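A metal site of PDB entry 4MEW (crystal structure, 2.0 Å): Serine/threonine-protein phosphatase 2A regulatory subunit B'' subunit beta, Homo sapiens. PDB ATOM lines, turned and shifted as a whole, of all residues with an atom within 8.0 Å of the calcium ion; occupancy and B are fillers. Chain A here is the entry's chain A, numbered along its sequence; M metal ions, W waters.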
ATOM      1  N   PHE A 196      18.141 -31.637 -25.605  1.00  0.00           N
ATOM      2  CA  PHE A 196      18.747 -30.558 -26.379  1.00  0.00           C
ATOM      3  C   PHE A 196      18.715 -29.266 -25.565  1.00  0.00           C
ATOM      4  O   PHE A 196      19.703 -28.530 -25.490  1.00  0.00           O
ATOM      5  CB  PHE A 196      18.002 -30.349 -27.701  1.00  0.00           C
ATOM      6  CG  PHE A 196      18.578 -29.259 -28.561  1.00  0.00           C
ATOM      7  CD1 PHE A 196      19.738 -29.480 -29.296  1.00  0.00           C
ATOM      8  CD2 PHE A 196      17.971 -28.021 -28.650  1.00  0.00           C
ATOM      9  CE1 PHE A 196      20.290 -28.479 -30.091  1.00  0.00           C
ATOM     10  CE2 PHE A 196      18.501 -27.016 -29.447  1.00  0.00           C
ATOM     11  CZ  PHE A 196      19.654 -27.245 -30.174  1.00  0.00           C
ATOM     12  N   LEU A 199      21.388 -28.527 -23.065  1.00  0.00           N
ATOM     13  CA  LEU A 199      22.686 -28.183 -23.623  1.00  0.00           C
ATOM     14  C   LEU A 199      22.710 -26.759 -24.173  1.00  0.00           C
ATOM     15  O   LEU A 199      23.713 -26.054 -24.046  1.00  0.00           O
ATOM     16  CB  LEU A 199      23.051 -29.169 -24.735  1.00  0.00           C
ATOM     17  CG  LEU A 199      23.207 -30.635 -24.304  1.00  0.00           C
ATOM     18  CD1 LEU A 199      23.515 -31.507 -25.499  1.00  0.00           C
ATOM     19  CD2 LEU A 199      24.298 -30.768 -23.253  1.00  0.00           C
ATOM     20  N   ASP A 200      21.600 -26.339 -24.769  1.00  0.00           N
ATOM     21  CA  ASP A 200      21.521 -25.029 -25.413  1.00  0.00           C
ATOM     22  C   ASP A 200      21.275 -23.924 -24.384  1.00  0.00           C
ATOM     23  O   ASP A 200      20.178 -23.378 -24.295  1.00  0.00           O
ATOM     24  CB  ASP A 200      20.422 -25.040 -26.471  1.00  0.00           C
ATOM     25  CG  ASP A 200      20.338 -23.733 -27.245  1.00  0.00           C
ATOM     26  OD1 ASP A 200      21.369 -23.046 -27.356  1.00  0.00           O
ATOM     27  OD2 ASP A 200      19.235 -23.409 -27.732  1.00  0.00           O
ATOM     28  N   THR A 201      22.305 -23.597 -23.612  1.00  0.00           N
ATOM     29  CA  THR A 201      22.116 -22.733 -22.443  1.00  0.00           C
ATOM     30  C   THR A 201      21.897 -21.250 -22.765  1.00  0.00           C
ATOM     31  O   THR A 201      21.425 -20.500 -21.919  1.00  0.00           O
ATOM     32  CB  THR A 201      23.267 -22.884 -21.420  1.00  0.00           C
ATOM     33  OG1 THR A 201      24.518 -22.590 -22.050  1.00  0.00           O
ATOM     34  CG2 THR A 201      23.314 -24.297 -20.869  1.00  0.00           C
ATOM     35  N   ASP A 202      22.222 -20.826 -23.988  1.00  0.00           N
ATOM     36  CA  ASP A 202      22.016 -19.423 -24.362  1.00  0.00           C
ATOM     37  C   ASP A 202      20.820 -19.272 -25.303  1.00  0.00           C
ATOM     38  O   ASP A 202      20.532 -18.168 -25.770  1.00  0.00           O
ATOM     39  CB  ASP A 202      23.283 -18.815 -24.962  1.00  0.00           C
ATOM     40  CG  ASP A 202      23.694 -19.460 -26.280  1.00  0.00           C
ATOM     41  OD1 ASP A 202      23.114 -20.504 -26.640  1.00  0.00           O
ATOM     42  OD2 ASP A 202      24.607 -18.919 -26.947  1.00  0.00           O
ATOM     43  N   HIS A 203      20.148 -20.389 -25.567  1.00  0.00           N
ATOM     44  CA  HIS A 203      18.871 -20.414 -26.284  1.00  0.00           C
ATOM     45  C   HIS A 203      18.908 -19.975 -27.743  1.00  0.00           C
ATOM     46  O   HIS A 203      17.891 -19.540 -28.277  1.00  0.00           O
ATOM     47  CB  HIS A 203      17.819 -19.583 -25.529  1.00  0.00           C
ATOM     48  CG  HIS A 203      17.677 -19.958 -24.080  1.00  0.00           C
ATOM     49  ND1 HIS A 203      18.335 -19.284 -23.072  1.00  0.00           N
ATOM     50  CD2 HIS A 203      16.959 -20.924 -23.465  1.00  0.00           C
ATOM     51  CE1 HIS A 203      18.027 -19.822 -21.910  1.00  0.00           C
ATOM     52  NE2 HIS A 203      17.189 -20.817 -22.125  1.00  0.00           N
ATOM     53  N   ASP A 204      20.046 -20.104 -28.410  1.00  0.00           N
ATOM     54  CA  ASP A 204      20.123 -19.722 -29.822  1.00  0.00           C
ATOM     55  C   ASP A 204      19.815 -20.880 -30.774  1.00  0.00           C
ATOM     56  O   ASP A 204      19.975 -20.761 -31.987  1.00  0.00           O
ATOM     57  CB  ASP A 204      21.475 -19.060 -30.154  1.00  0.00           C
ATOM     58  CG  ASP A 204      22.631 -20.052 -30.217  1.00  0.00           C
ATOM     59  OD1 ASP A 204      22.446 -21.210 -29.783  1.00  0.00           O
ATOM     60  OD2 ASP A 204      23.722 -19.667 -30.692  1.00  0.00           O
ATOM     61  N   LEU A 205      19.374 -22.003 -30.197  1.00  0.00           N
ATOM     62  CA  LEU A 205      18.983 -23.207 -30.931  1.00  0.00           C
ATOM     63  C   LEU A 205      20.151 -23.894 -31.659  1.00  0.00           C
ATOM     64  O   LEU A 205      19.955 -24.749 -32.522  1.00  0.00           O
ATOM     65  CB  LEU A 205      17.831 -22.918 -31.902  1.00  0.00           C
ATOM     66  CG  LEU A 205      16.636 -22.190 -31.275  1.00  0.00           C
ATOM     67  CD1 LEU A 205      15.474 -22.096 -32.248  1.00  0.00           C
ATOM     68  CD2 LEU A 205      16.195 -22.876 -29.977  1.00  0.00           C
ATOM     69  N   LEU A 206      21.374 -23.524 -31.279  1.00  0.00           N
ATOM     70  CA  LEU A 206      22.571 -24.158 -31.815  1.00  0.00           C
ATOM     71  C   LEU A 206      23.441 -24.622 -30.650  1.00  0.00           C
ATOM     72  O   LEU A 206      23.461 -23.988 -29.611  1.00  0.00           O
ATOM     73  CB  LEU A 206      23.361 -23.167 -32.668  1.00  0.00           C
ATOM     74  CG  LEU A 206      22.656 -22.613 -33.920  1.00  0.00           C
ATOM     75  CD1 LEU A 206      23.537 -21.562 -34.579  1.00  0.00           C
ATOM     76  CD2 LEU A 206      22.326 -23.730 -34.894  1.00  0.00           C
ATOM     77  N   ILE A 207      24.167 -25.725 -30.832  1.00  0.00           N
ATOM     78  CA  ILE A 207      25.113 -26.130 -29.803  1.00  0.00           C
ATOM     79  C   ILE A 207      26.498 -26.337 -30.389  1.00  0.00           C
ATOM     80  O   ILE A 207      26.639 -26.721 -31.549  1.00  0.00           O
ATOM     81  CB  ILE A 207      24.652 -27.388 -29.027  1.00  0.00           C
ATOM     82  CG1 ILE A 207      24.404 -28.551 -29.992  1.00  0.00           C
ATOM     83  CG2 ILE A 207      23.401 -27.088 -28.211  1.00  0.00           C
ATOM     84  CD1 ILE A 207      23.974 -29.827 -29.282  1.00  0.00           C
ATOM     85  N   ASP A 208      27.514 -26.065 -29.581  1.00  0.00           N
ATOM     86  CA  ASP A 208      28.889 -26.237 -30.025  1.00  0.00           C
ATOM     87  C   ASP A 208      29.526 -27.487 -29.437  1.00  0.00           C
ATOM     88  O   ASP A 208      28.862 -28.291 -28.780  1.00  0.00           O
ATOM     89  CB  ASP A 208      29.727 -24.968 -29.743  1.00  0.00           C
ATOM     90  CG  ASP A 208      29.906 -24.681 -28.251  1.00  0.00           C
ATOM     91  OD1 ASP A 208      29.654 -25.576 -27.418  1.00  0.00           O
ATOM     92  OD2 ASP A 208      30.334 -23.557 -27.913  1.00  0.00           O
ATOM     93  N   ASP A 211      29.343 -27.737 -25.613  1.00  0.00           N
ATOM     94  CA  ASP A 211      28.001 -28.145 -25.224  1.00  0.00           C
ATOM     95  C   ASP A 211      27.813 -29.656 -25.411  1.00  0.00           C
ATOM     96  O   ASP A 211      27.413 -30.359 -24.486  1.00  0.00           O
ATOM     97  CB  ASP A 211      26.929 -27.412 -26.041  1.00  0.00           C
ATOM     98  CG  ASP A 211      27.014 -25.904 -25.912  1.00  0.00           C
ATOM     99  OD1 ASP A 211      27.327 -25.404 -24.812  1.00  0.00           O
ATOM    100  OD2 ASP A 211      26.750 -25.221 -26.916  1.00  0.00           O
ATOM    101  N   ARG A 214      29.262 -32.069 -22.927  1.00  0.00           N
ATOM    102  CA  ARG A 214      28.541 -32.169 -21.659  1.00  0.00           C
ATOM    103  C   ARG A 214      27.484 -33.273 -21.661  1.00  0.00           C
ATOM    104  O   ARG A 214      27.168 -33.831 -20.614  1.00  0.00           O
ATOM    105  CB  ARG A 214      27.882 -30.828 -21.304  1.00  0.00           C
ATOM    106  CG  ARG A 214      28.839 -29.762 -20.798  1.00  0.00           C
ATOM    107  CD  ARG A 214      28.089 -28.536 -20.272  1.00  0.00           C
ATOM    108  NE  ARG A 214      27.636 -27.653 -21.333  1.00  0.00           N
ATOM    109  CZ  ARG A 214      26.367 -27.326 -21.560  1.00  0.00           C
ATOM    110  NH1 ARG A 214      25.406 -27.819 -20.786  1.00  0.00           N
ATOM    111  NH2 ARG A 214      26.053 -26.515 -22.554  1.00  0.00           N
ATOM    112  N   LYS A 244      29.047 -25.249 -35.060  1.00  0.00           N
ATOM    113  CA  LYS A 244      27.787 -25.444 -34.343  1.00  0.00           C
ATOM    114  C   LYS A 244      26.879 -26.384 -35.119  1.00  0.00           C
ATOM    115  O   LYS A 244      26.916 -26.418 -36.352  1.00  0.00           O
ATOM    116  CB  LYS A 244      27.083 -24.098 -34.108  1.00  0.00           C
ATOM    117  CG  LYS A 244      27.852 -23.130 -33.228  1.00  0.00           C
ATOM    118  CD  LYS A 244      26.931 -22.118 -32.598  1.00  0.00           C
ATOM    119  CE  LYS A 244      27.662 -21.248 -31.579  1.00  0.00           C
ATOM    120  NZ  LYS A 244      26.694 -20.412 -30.819  1.00  0.00           N
ATOM    121  N   ILE A 245      26.089 -27.163 -34.398  1.00  0.00           N
ATOM    122  CA  ILE A 245      25.090 -28.021 -35.042  1.00  0.00           C
ATOM    123  C   ILE A 245      23.700 -27.630 -34.588  1.00  0.00           C
ATOM    124  O   ILE A 245      23.516 -27.043 -33.523  1.00  0.00           O
ATOM    125  CB  ILE A 245      25.315 -29.521 -34.757  1.00  0.00           C
ATOM    126  CG1 ILE A 245      25.176 -29.798 -33.261  1.00  0.00           C
ATOM    127  CG2 ILE A 245      26.666 -29.980 -35.308  1.00  0.00           C
ATOM    128  CD1 ILE A 245      25.022 -31.265 -32.931  1.00  0.00           C
HETATM  129 CA    CA M   1      23.445 -22.370 -28.086  1.00  0.00          CA
HETATM  130  O   HOH W   1      24.533 -23.536 -26.415  1.00  0.00           O
HETATM  131  O   HOH W   2      25.646 -21.112 -28.533  1.00  0.00           O
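The backbone NH of His 203 lies close to the side-chain carboxylate of Asp 200, at 3.4 Å.
N of Leu 205 is in hydrogen-bond range of OD2 of Asp 200 (2.8 Å).
The side-chain amino group (NZ) of Lys 244 is in salt-bridge range of the side-chain carboxylate (OD2) of Asp 204, at 3.1 Å.
Of the 15 residues printed, 4 come within 4 Å of the calcium ion.
Along chain A the residues within 4 Å of the calcium ion span positions 200 to 206.
The backbone carbonyl oxygen (O) of Leu 206 is bound to the calcium ion, at 2.2 Å.
The calcium ion is bound by OD1 of Asp 204, 2.3 Å away.
The side-chain carboxylate (OD1) of Asp 200 binds the calcium ion (2.3 Å).
Water W1 is bound to the calcium ion.
The calcium ion is bound by OD1 of Asp 202 (2.4 Å).
The calcium ion is bound by water W2 (2.6 Å).
The calcium ion has six donor atoms within binding distance.
Water W2 lies within hydrogen-bond range of the side-chain amino group of Lys 244, the side-chain carboxylate of Asp 202 and the side-chain carboxylate of Asp 204.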
